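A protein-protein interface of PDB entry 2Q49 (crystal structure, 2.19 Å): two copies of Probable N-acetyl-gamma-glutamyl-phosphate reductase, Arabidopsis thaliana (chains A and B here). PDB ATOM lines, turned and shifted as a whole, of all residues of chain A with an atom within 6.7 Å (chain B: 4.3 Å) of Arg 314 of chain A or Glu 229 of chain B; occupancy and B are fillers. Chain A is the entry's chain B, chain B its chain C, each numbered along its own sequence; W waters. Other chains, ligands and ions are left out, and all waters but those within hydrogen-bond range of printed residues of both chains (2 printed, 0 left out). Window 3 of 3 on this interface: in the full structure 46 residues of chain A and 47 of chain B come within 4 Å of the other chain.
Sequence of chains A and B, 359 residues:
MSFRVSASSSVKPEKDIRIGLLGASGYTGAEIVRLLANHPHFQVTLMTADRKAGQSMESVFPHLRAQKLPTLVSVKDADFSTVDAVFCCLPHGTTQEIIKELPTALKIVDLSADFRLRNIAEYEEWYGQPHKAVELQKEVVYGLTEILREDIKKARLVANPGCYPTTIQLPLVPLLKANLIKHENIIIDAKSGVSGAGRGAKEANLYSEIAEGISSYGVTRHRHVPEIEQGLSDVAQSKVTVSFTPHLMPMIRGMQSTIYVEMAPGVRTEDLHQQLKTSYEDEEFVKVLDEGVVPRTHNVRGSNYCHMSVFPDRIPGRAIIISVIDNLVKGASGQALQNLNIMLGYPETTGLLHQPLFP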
ATOM      1  N   PRO A 312     -18.264  31.731  -1.960  1.00  0.00           N
ATOM      2  CA  PRO A 312     -17.225  31.928  -0.957  1.00  0.00           C
ATOM      3  C   PRO A 312     -15.854  31.988  -1.652  1.00  0.00           C
ATOM      4  O   PRO A 312     -15.647  31.393  -2.721  1.00  0.00           O
ATOM      5  CB  PRO A 312     -17.367  30.691  -0.075  1.00  0.00           C
ATOM      6  CG  PRO A 312     -17.801  29.651  -1.057  1.00  0.00           C
ATOM      7  CD  PRO A 312     -18.851  30.386  -1.847  1.00  0.00           C
ATOM      8  N   ASP A 313     -14.942  32.738  -1.049  1.00  0.00           N
ATOM      9  CA  ASP A 313     -13.594  32.853  -1.544  1.00  0.00           C
ATOM     10  C   ASP A 313     -12.801  31.760  -0.821  1.00  0.00           C
ATOM     11  O   ASP A 313     -13.139  31.365   0.303  1.00  0.00           O
ATOM     12  CB  ASP A 313     -13.012  34.233  -1.220  1.00  0.00           C
ATOM     13  CG  ASP A 313     -11.724  34.517  -1.986  1.00  0.00           C
ATOM     14  OD1 ASP A 313     -10.662  33.992  -1.585  1.00  0.00           O
ATOM     15  OD2 ASP A 313     -11.777  35.263  -2.999  1.00  0.00           O
ATOM     16  N   ARG A 314     -11.764  31.251  -1.467  1.00  0.00           N
ATOM     17  CA  ARG A 314     -10.947  30.216  -0.851  1.00  0.00           C
ATOM     18  C   ARG A 314     -10.250  30.845   0.352  1.00  0.00           C
ATOM     19  O   ARG A 314      -9.954  30.172   1.338  1.00  0.00           O
ATOM     20  CB  ARG A 314      -9.918  29.690  -1.861  1.00  0.00           C
ATOM     21  CG  ARG A 314      -8.982  28.635  -1.318  1.00  0.00           C
ATOM     22  CD  ARG A 314      -8.063  28.111  -2.423  1.00  0.00           C
ATOM     23  NE  ARG A 314      -7.035  27.206  -1.928  1.00  0.00           N
ATOM     24  CZ  ARG A 314      -7.267  26.006  -1.401  1.00  0.00           C
ATOM     25  NH1 ARG A 314      -8.507  25.542  -1.288  1.00  0.00           N
ATOM     26  NH2 ARG A 314      -6.250  25.259  -0.993  1.00  0.00           N
ATOM     27  N   ILE A 315      -9.981  32.143   0.259  1.00  0.00           N
ATOM     28  CA  ILE A 315      -9.341  32.857   1.355  1.00  0.00           C
ATOM     29  C   ILE A 315     -10.404  33.061   2.439  1.00  0.00           C
ATOM     30  O   ILE A 315     -11.406  33.732   2.219  1.00  0.00           O
ATOM     31  CB  ILE A 315      -8.789  34.244   0.898  1.00  0.00           C
ATOM     32  CG1 ILE A 315      -7.568  34.060  -0.012  1.00  0.00           C
ATOM     33  CG2 ILE A 315      -8.382  35.075   2.113  1.00  0.00           C
ATOM     34  CD1 ILE A 315      -7.027  35.375  -0.579  1.00  0.00           C
ATOM     35  N   PRO A 316     -10.213  32.454   3.617  1.00  0.00           N
ATOM     36  CA  PRO A 316     -11.202  32.609   4.697  1.00  0.00           C
ATOM     37  C   PRO A 316     -11.587  34.075   4.965  1.00  0.00           C
ATOM     38  O   PRO A 316     -10.731  34.963   5.004  1.00  0.00           O
ATOM     39  CB  PRO A 316     -10.508  31.954   5.890  1.00  0.00           C
ATOM     40  CG  PRO A 316      -9.710  30.841   5.227  1.00  0.00           C
ATOM     41  CD  PRO A 316      -9.132  31.527   4.002  1.00  0.00           C
ATOM     42  N   GLY A 317     -12.882  34.318   5.126  1.00  0.00           N
ATOM     43  CA  GLY A 317     -13.348  35.661   5.386  1.00  0.00           C
ATOM     44  C   GLY A 317     -13.770  36.421   4.146  1.00  0.00           C
ATOM     45  O   GLY A 317     -14.481  37.419   4.237  1.00  0.00           O
ATOM     46  N   ARG A 318     -13.346  35.947   2.981  1.00  0.00           N
ATOM     47  CA  ARG A 318     -13.681  36.615   1.740  1.00  0.00           C
ATOM     48  C   ARG A 318     -14.820  35.942   0.982  1.00  0.00           C
ATOM     49  O   ARG A 318     -15.155  34.788   1.254  1.00  0.00           O
ATOM     50  CB  ARG A 318     -12.427  36.723   0.860  1.00  0.00           C
ATOM     51  CG  ARG A 318     -11.678  38.007   1.104  1.00  0.00           C
ATOM     52  CD  ARG A 318     -10.446  38.166   0.227  1.00  0.00           C
ATOM     53  NE  ARG A 318      -9.938  39.526   0.344  1.00  0.00           N
ATOM     54  CZ  ARG A 318     -10.416  40.555  -0.345  1.00  0.00           C
ATOM     55  NH1 ARG A 318     -11.406  40.373  -1.215  1.00  0.00           N
ATOM     56  NH2 ARG A 318      -9.919  41.772  -0.148  1.00  0.00           N
ATOM     57  N   ILE A 320     -17.036  36.037  -3.131  1.00  0.00           N
ATOM     58  CA  ILE A 320     -16.997  36.452  -4.525  1.00  0.00           C
ATOM     59  C   ILE A 320     -18.387  36.851  -4.969  1.00  0.00           C
ATOM     60  O   ILE A 320     -19.365  36.129  -4.718  1.00  0.00           O
ATOM     61  CB  ILE A 320     -16.534  35.333  -5.472  1.00  0.00           C
ATOM     62  CG1 ILE A 320     -15.078  34.963  -5.199  1.00  0.00           C
ATOM     63  CG2 ILE A 320     -16.701  35.790  -6.906  1.00  0.00           C
ATOM     64  CD1 ILE A 320     -14.650  33.655  -5.873  1.00  0.00           C
ATOM     65  N   TRP B 126      -7.916  16.420  -4.133  1.00  0.00           N
ATOM     66  CA  TRP B 126      -8.299  17.216  -5.291  1.00  0.00           C
ATOM     67  C   TRP B 126      -8.575  16.409  -6.535  1.00  0.00           C
ATOM     68  O   TRP B 126      -8.894  16.976  -7.583  1.00  0.00           O
ATOM     69  CB  TRP B 126      -7.222  18.241  -5.616  1.00  0.00           C
ATOM     70  CG  TRP B 126      -7.158  19.360  -4.654  1.00  0.00           C
ATOM     71  CD1 TRP B 126      -6.431  19.411  -3.512  1.00  0.00           C
ATOM     72  CD2 TRP B 126      -7.863  20.597  -4.742  1.00  0.00           C
ATOM     73  NE1 TRP B 126      -6.630  20.604  -2.876  1.00  0.00           N
ATOM     74  CE2 TRP B 126      -7.509  21.356  -3.610  1.00  0.00           C
ATOM     75  CE3 TRP B 126      -8.762  21.140  -5.671  1.00  0.00           C
ATOM     76  CZ2 TRP B 126      -8.019  22.638  -3.373  1.00  0.00           C
ATOM     77  CZ3 TRP B 126      -9.273  22.420  -5.436  1.00  0.00           C
ATOM     78  CH2 TRP B 126      -8.898  23.151  -4.295  1.00  0.00           C
ATOM     79  N   THR B 220     -13.985  29.189  -6.298  1.00  0.00           N
ATOM     80  CA  THR B 220     -13.623  28.672  -4.981  1.00  0.00           C
ATOM     81  C   THR B 220     -12.663  27.495  -5.049  1.00  0.00           C
ATOM     82  O   THR B 220     -11.649  27.478  -4.357  1.00  0.00           O
ATOM     83  CB  THR B 220     -14.840  28.177  -4.188  1.00  0.00           C
ATOM     84  OG1 THR B 220     -15.886  29.156  -4.239  1.00  0.00           O
ATOM     85  CG2 THR B 220     -14.434  27.915  -2.740  1.00  0.00           C
ATOM     86  N   VAL B 225      -5.608  25.022  -8.198  1.00  0.00           N
ATOM     87  CA  VAL B 225      -5.367  25.664  -6.901  1.00  0.00           C
ATOM     88  C   VAL B 225      -4.207  25.013  -6.129  1.00  0.00           C
ATOM     89  O   VAL B 225      -3.227  25.702  -5.820  1.00  0.00           O
ATOM     90  CB  VAL B 225      -6.675  25.717  -6.038  1.00  0.00           C
ATOM     91  CG1 VAL B 225      -6.366  26.190  -4.620  1.00  0.00           C
ATOM     92  CG2 VAL B 225      -7.684  26.674  -6.679  1.00  0.00           C
ATOM     93  N   PRO B 226      -4.274  23.689  -5.833  1.00  0.00           N
ATOM     94  CA  PRO B 226      -3.152  23.077  -5.095  1.00  0.00           C
ATOM     95  C   PRO B 226      -1.802  23.212  -5.811  1.00  0.00           C
ATOM     96  O   PRO B 226      -0.768  23.425  -5.163  1.00  0.00           O
ATOM     97  CB  PRO B 226      -3.588  21.612  -4.912  1.00  0.00           C
ATOM     98  CG  PRO B 226      -4.591  21.383  -6.031  1.00  0.00           C
ATOM     99  CD  PRO B 226      -5.332  22.695  -6.101  1.00  0.00           C
ATOM    100  N   GLU B 227      -1.822  23.097  -7.143  1.00  0.00           N
ATOM    101  CA  GLU B 227      -0.614  23.237  -7.969  1.00  0.00           C
ATOM    102  C   GLU B 227       0.000  24.634  -7.794  1.00  0.00           C
ATOM    103  O   GLU B 227       1.215  24.780  -7.594  1.00  0.00           O
ATOM    104  CB  GLU B 227      -0.963  23.043  -9.446  1.00  0.00           C
ATOM    105  CG  GLU B 227       0.250  22.962 -10.357  1.00  0.00           C
ATOM    106  CD  GLU B 227      -0.120  22.872 -11.807  1.00  0.00           C
ATOM    107  OE1 GLU B 227      -1.256  22.427 -12.104  1.00  0.00           O
ATOM    108  OE2 GLU B 227       0.729  23.232 -12.656  1.00  0.00           O
ATOM    109  N   ILE B 228      -0.852  25.658  -7.890  1.00  0.00           N
ATOM    110  CA  ILE B 228      -0.429  27.044  -7.720  1.00  0.00           C
ATOM    111  C   ILE B 228       0.120  27.271  -6.309  1.00  0.00           C
ATOM    112  O   ILE B 228       1.226  27.773  -6.134  1.00  0.00           O
ATOM    113  CB  ILE B 228      -1.621  28.050  -7.952  1.00  0.00           C
ATOM    114  CG1 ILE B 228      -2.114  27.992  -9.402  1.00  0.00           C
ATOM    115  CG2 ILE B 228      -1.165  29.491  -7.639  1.00  0.00           C
ATOM    116  CD1 ILE B 228      -3.508  28.638  -9.587  1.00  0.00           C
ATOM    117  N   GLU B 229      -0.652  26.884  -5.297  1.00  0.00           N
ATOM    118  CA  GLU B 229      -0.225  27.088  -3.914  1.00  0.00           C
ATOM    119  C   GLU B 229       1.076  26.349  -3.566  1.00  0.00           C
ATOM    120  O   GLU B 229       1.939  26.905  -2.868  1.00  0.00           O
ATOM    121  CB  GLU B 229      -1.358  26.706  -2.948  1.00  0.00           C
ATOM    122  CG  GLU B 229      -2.638  27.549  -3.168  1.00  0.00           C
ATOM    123  CD  GLU B 229      -3.721  27.350  -2.104  1.00  0.00           C
ATOM    124  OE1 GLU B 229      -3.773  26.264  -1.493  1.00  0.00           O
ATOM    125  OE2 GLU B 229      -4.535  28.283  -1.895  1.00  0.00           O
ATOM    126  N   GLN B 230       1.241  25.122  -4.057  1.00  0.00           N
ATOM    127  CA  GLN B 230       2.472  24.372  -3.768  1.00  0.00           C
ATOM    128  C   GLN B 230       3.689  25.117  -4.316  1.00  0.00           C
ATOM    129  O   GLN B 230       4.731  25.211  -3.654  1.00  0.00           O
ATOM    130  CB  GLN B 230       2.416  22.967  -4.384  1.00  0.00           C
ATOM    131  CG  GLN B 230       3.700  22.135  -4.178  1.00  0.00           C
ATOM    132  CD  GLN B 230       3.511  20.680  -4.588  1.00  0.00           C
ATOM    133  OE1 GLN B 230       2.852  19.887  -3.886  1.00  0.00           O
ATOM    134  NE2 GLN B 230       4.072  20.322  -5.735  1.00  0.00           N
ATOM    135  N   GLY B 231       3.551  25.632  -5.536  1.00  0.00           N
ATOM    136  CA  GLY B 231       4.628  26.383  -6.158  1.00  0.00           C
ATOM    137  C   GLY B 231       4.952  27.638  -5.360  1.00  0.00           C
ATOM    138  O   GLY B 231       6.126  27.938  -5.102  1.00  0.00           O
ATOM    139  N   LEU B 232       3.914  28.380  -4.971  1.00  0.00           N
ATOM    140  CA  LEU B 232       4.112  29.604  -4.193  1.00  0.00           C
ATOM    141  C   LEU B 232       4.570  29.292  -2.764  1.00  0.00           C
ATOM    142  O   LEU B 232       5.446  29.969  -2.217  1.00  0.00           O
ATOM    143  CB  LEU B 232       2.827  30.449  -4.150  1.00  0.00           C
ATOM    144  CG  LEU B 232       2.244  30.947  -5.488  1.00  0.00           C
ATOM    145  CD1 LEU B 232       1.224  32.049  -5.218  1.00  0.00           C
ATOM    146  CD2 LEU B 232       3.355  31.486  -6.389  1.00  0.00           C
ATOM    147  N   SER B 233       3.997  28.262  -2.160  1.00  0.00           N
ATOM    148  CA  SER B 233       4.380  27.913  -0.796  1.00  0.00           C
ATOM    149  C   SER B 233       5.843  27.479  -0.685  1.00  0.00           C
ATOM    150  O   SER B 233       6.531  27.814   0.296  1.00  0.00           O
ATOM    151  CB  SER B 233       3.450  26.824  -0.240  1.00  0.00           C
ATOM    152  OG  SER B 233       2.120  27.331  -0.123  1.00  0.00           O
ATOM    153  N   VAL B 240       0.857  28.974   1.540  1.00  0.00           N
ATOM    154  CA  VAL B 240       0.253  30.082   0.826  1.00  0.00           C
ATOM    155  C   VAL B 240      -1.123  29.702   0.307  1.00  0.00           C
ATOM    156  O   VAL B 240      -1.253  28.802  -0.521  1.00  0.00           O
ATOM    157  CB  VAL B 240       1.123  30.522  -0.371  1.00  0.00           C
ATOM    158  CG1 VAL B 240       0.324  31.442  -1.275  1.00  0.00           C
ATOM    159  CG2 VAL B 240       2.373  31.220   0.133  1.00  0.00           C
ATOM    160  N   THR B 241      -2.147  30.381   0.814  1.00  0.00           N
ATOM    161  CA  THR B 241      -3.526  30.155   0.382  1.00  0.00           C
ATOM    162  C   THR B 241      -3.926  31.346  -0.494  1.00  0.00           C
ATOM    163  O   THR B 241      -3.938  32.487  -0.032  1.00  0.00           O
ATOM    164  CB  THR B 241      -4.510  30.080   1.578  1.00  0.00           C
ATOM    165  OG1 THR B 241      -4.142  28.991   2.438  1.00  0.00           O
ATOM    166  CG2 THR B 241      -5.935  29.866   1.081  1.00  0.00           C
ATOM    167  N   VAL B 242      -4.246  31.074  -1.753  1.00  0.00           N
ATOM    168  CA  VAL B 242      -4.624  32.128  -2.682  1.00  0.00           C
ATOM    169  C   VAL B 242      -6.096  32.080  -3.074  1.00  0.00           C
ATOM    170  O   VAL B 242      -6.823  31.127  -2.758  1.00  0.00           O
ATOM    171  CB  VAL B 242      -3.795  32.039  -4.012  1.00  0.00           C
ATOM    172  CG1 VAL B 242      -2.317  31.887  -3.706  1.00  0.00           C
ATOM    173  CG2 VAL B 242      -4.299  30.873  -4.876  1.00  0.00           C
HETATM  174  O   HOH W   1     -10.952  26.520  -1.881  1.00  0.00           O
HETATM  175  O   HOH W   2      -5.298  22.013  -0.353  1.00  0.00           O
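The backbone carbonyl oxygen (O) of Pro 312 of chain A lies within hydrogen-bond range of the side-chain hydroxyl (OG1) of Thr 220 of chain B (2.7 Å).
The guanidinium group of Arg 314 of chain A is in salt-bridge range of the side-chain carboxylate of Glu 229 of chain B (2.7 Å).
N of Ile 315 of chain A sits at hydrogen-bond distance from OD1 of Asp 313 of chain A (2.7 Å).
The backbone carbonyl oxygen of Glu 229 of chain B lies within hydrogen-bond range of the side-chain hydroxyl of Ser 233 of chain B, 2.8 Å away.
OE2 of Glu 229 of chain B lies within hydrogen-bond range of N of Val 242 of chain B.
Among the printed residues, pairs that only touch across the chains: Arg 314 of chain A with Val 225 of chain B (3.0 Å), Arg 314 of chain A with Val 242 of chain B (3.3 Å), Arg 314 of chain A with Trp 126 of chain B (3.6 Å), Arg 314 of chain A with Thr 220 of chain B (3.8 Å), Ile 315 of chain A with Val 242 of chain B (3.9 Å) and Ile 315 of chain A with Thr 241 of chain B (3.96 Å).
Arg 314 of chain A touches just these residues of chain B: Trp 126, Thr 220, Val 225, Glu 229 and Val 242.
Of the printed residues of chain A, Thr 220 of chain B touches Pro 312 (2.7 Å) and Arg 314 (3.8 Å).
Printed residues of chain A within 4 Å of Val 225 of chain B: Arg 314 (3.0 Å).
Glu 227 of chain B touches none of the printed residues of chain A.
Glu 229 of chain B touches just one residue of chain A: Arg 314.
The nearest printed residue of chain A that does not touch Thr 220 of chain B is Ile 320 of chain A (4.5 Å).
Hydrophobic or aromatic side chains of chain A within 4 Å of the printed part of chain B: Pro 312 and Ile 315.
Of the 14 printed residues of chain B, 6 touch a printed residue of chain A.
Hydrophobic or aromatic side chains of chain B that line the printed part of chain A: Trp 126 and Val 225.
No position is printed for both chains.
Of the 8 pairs that touch across the chains among the printed residues, none has its exchanged pair printed and touching as well.
Water W1 lies within hydrogen-bond range of NH1 of Arg 314 of chain A and O of Thr 220 of chain B.
Water W2 lies within hydrogen-bond range of the indole nitrogen of Trp 126 of chain B (3.2 Å) and the guanidinium group of Arg 314 of chain A (3.4 Å).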
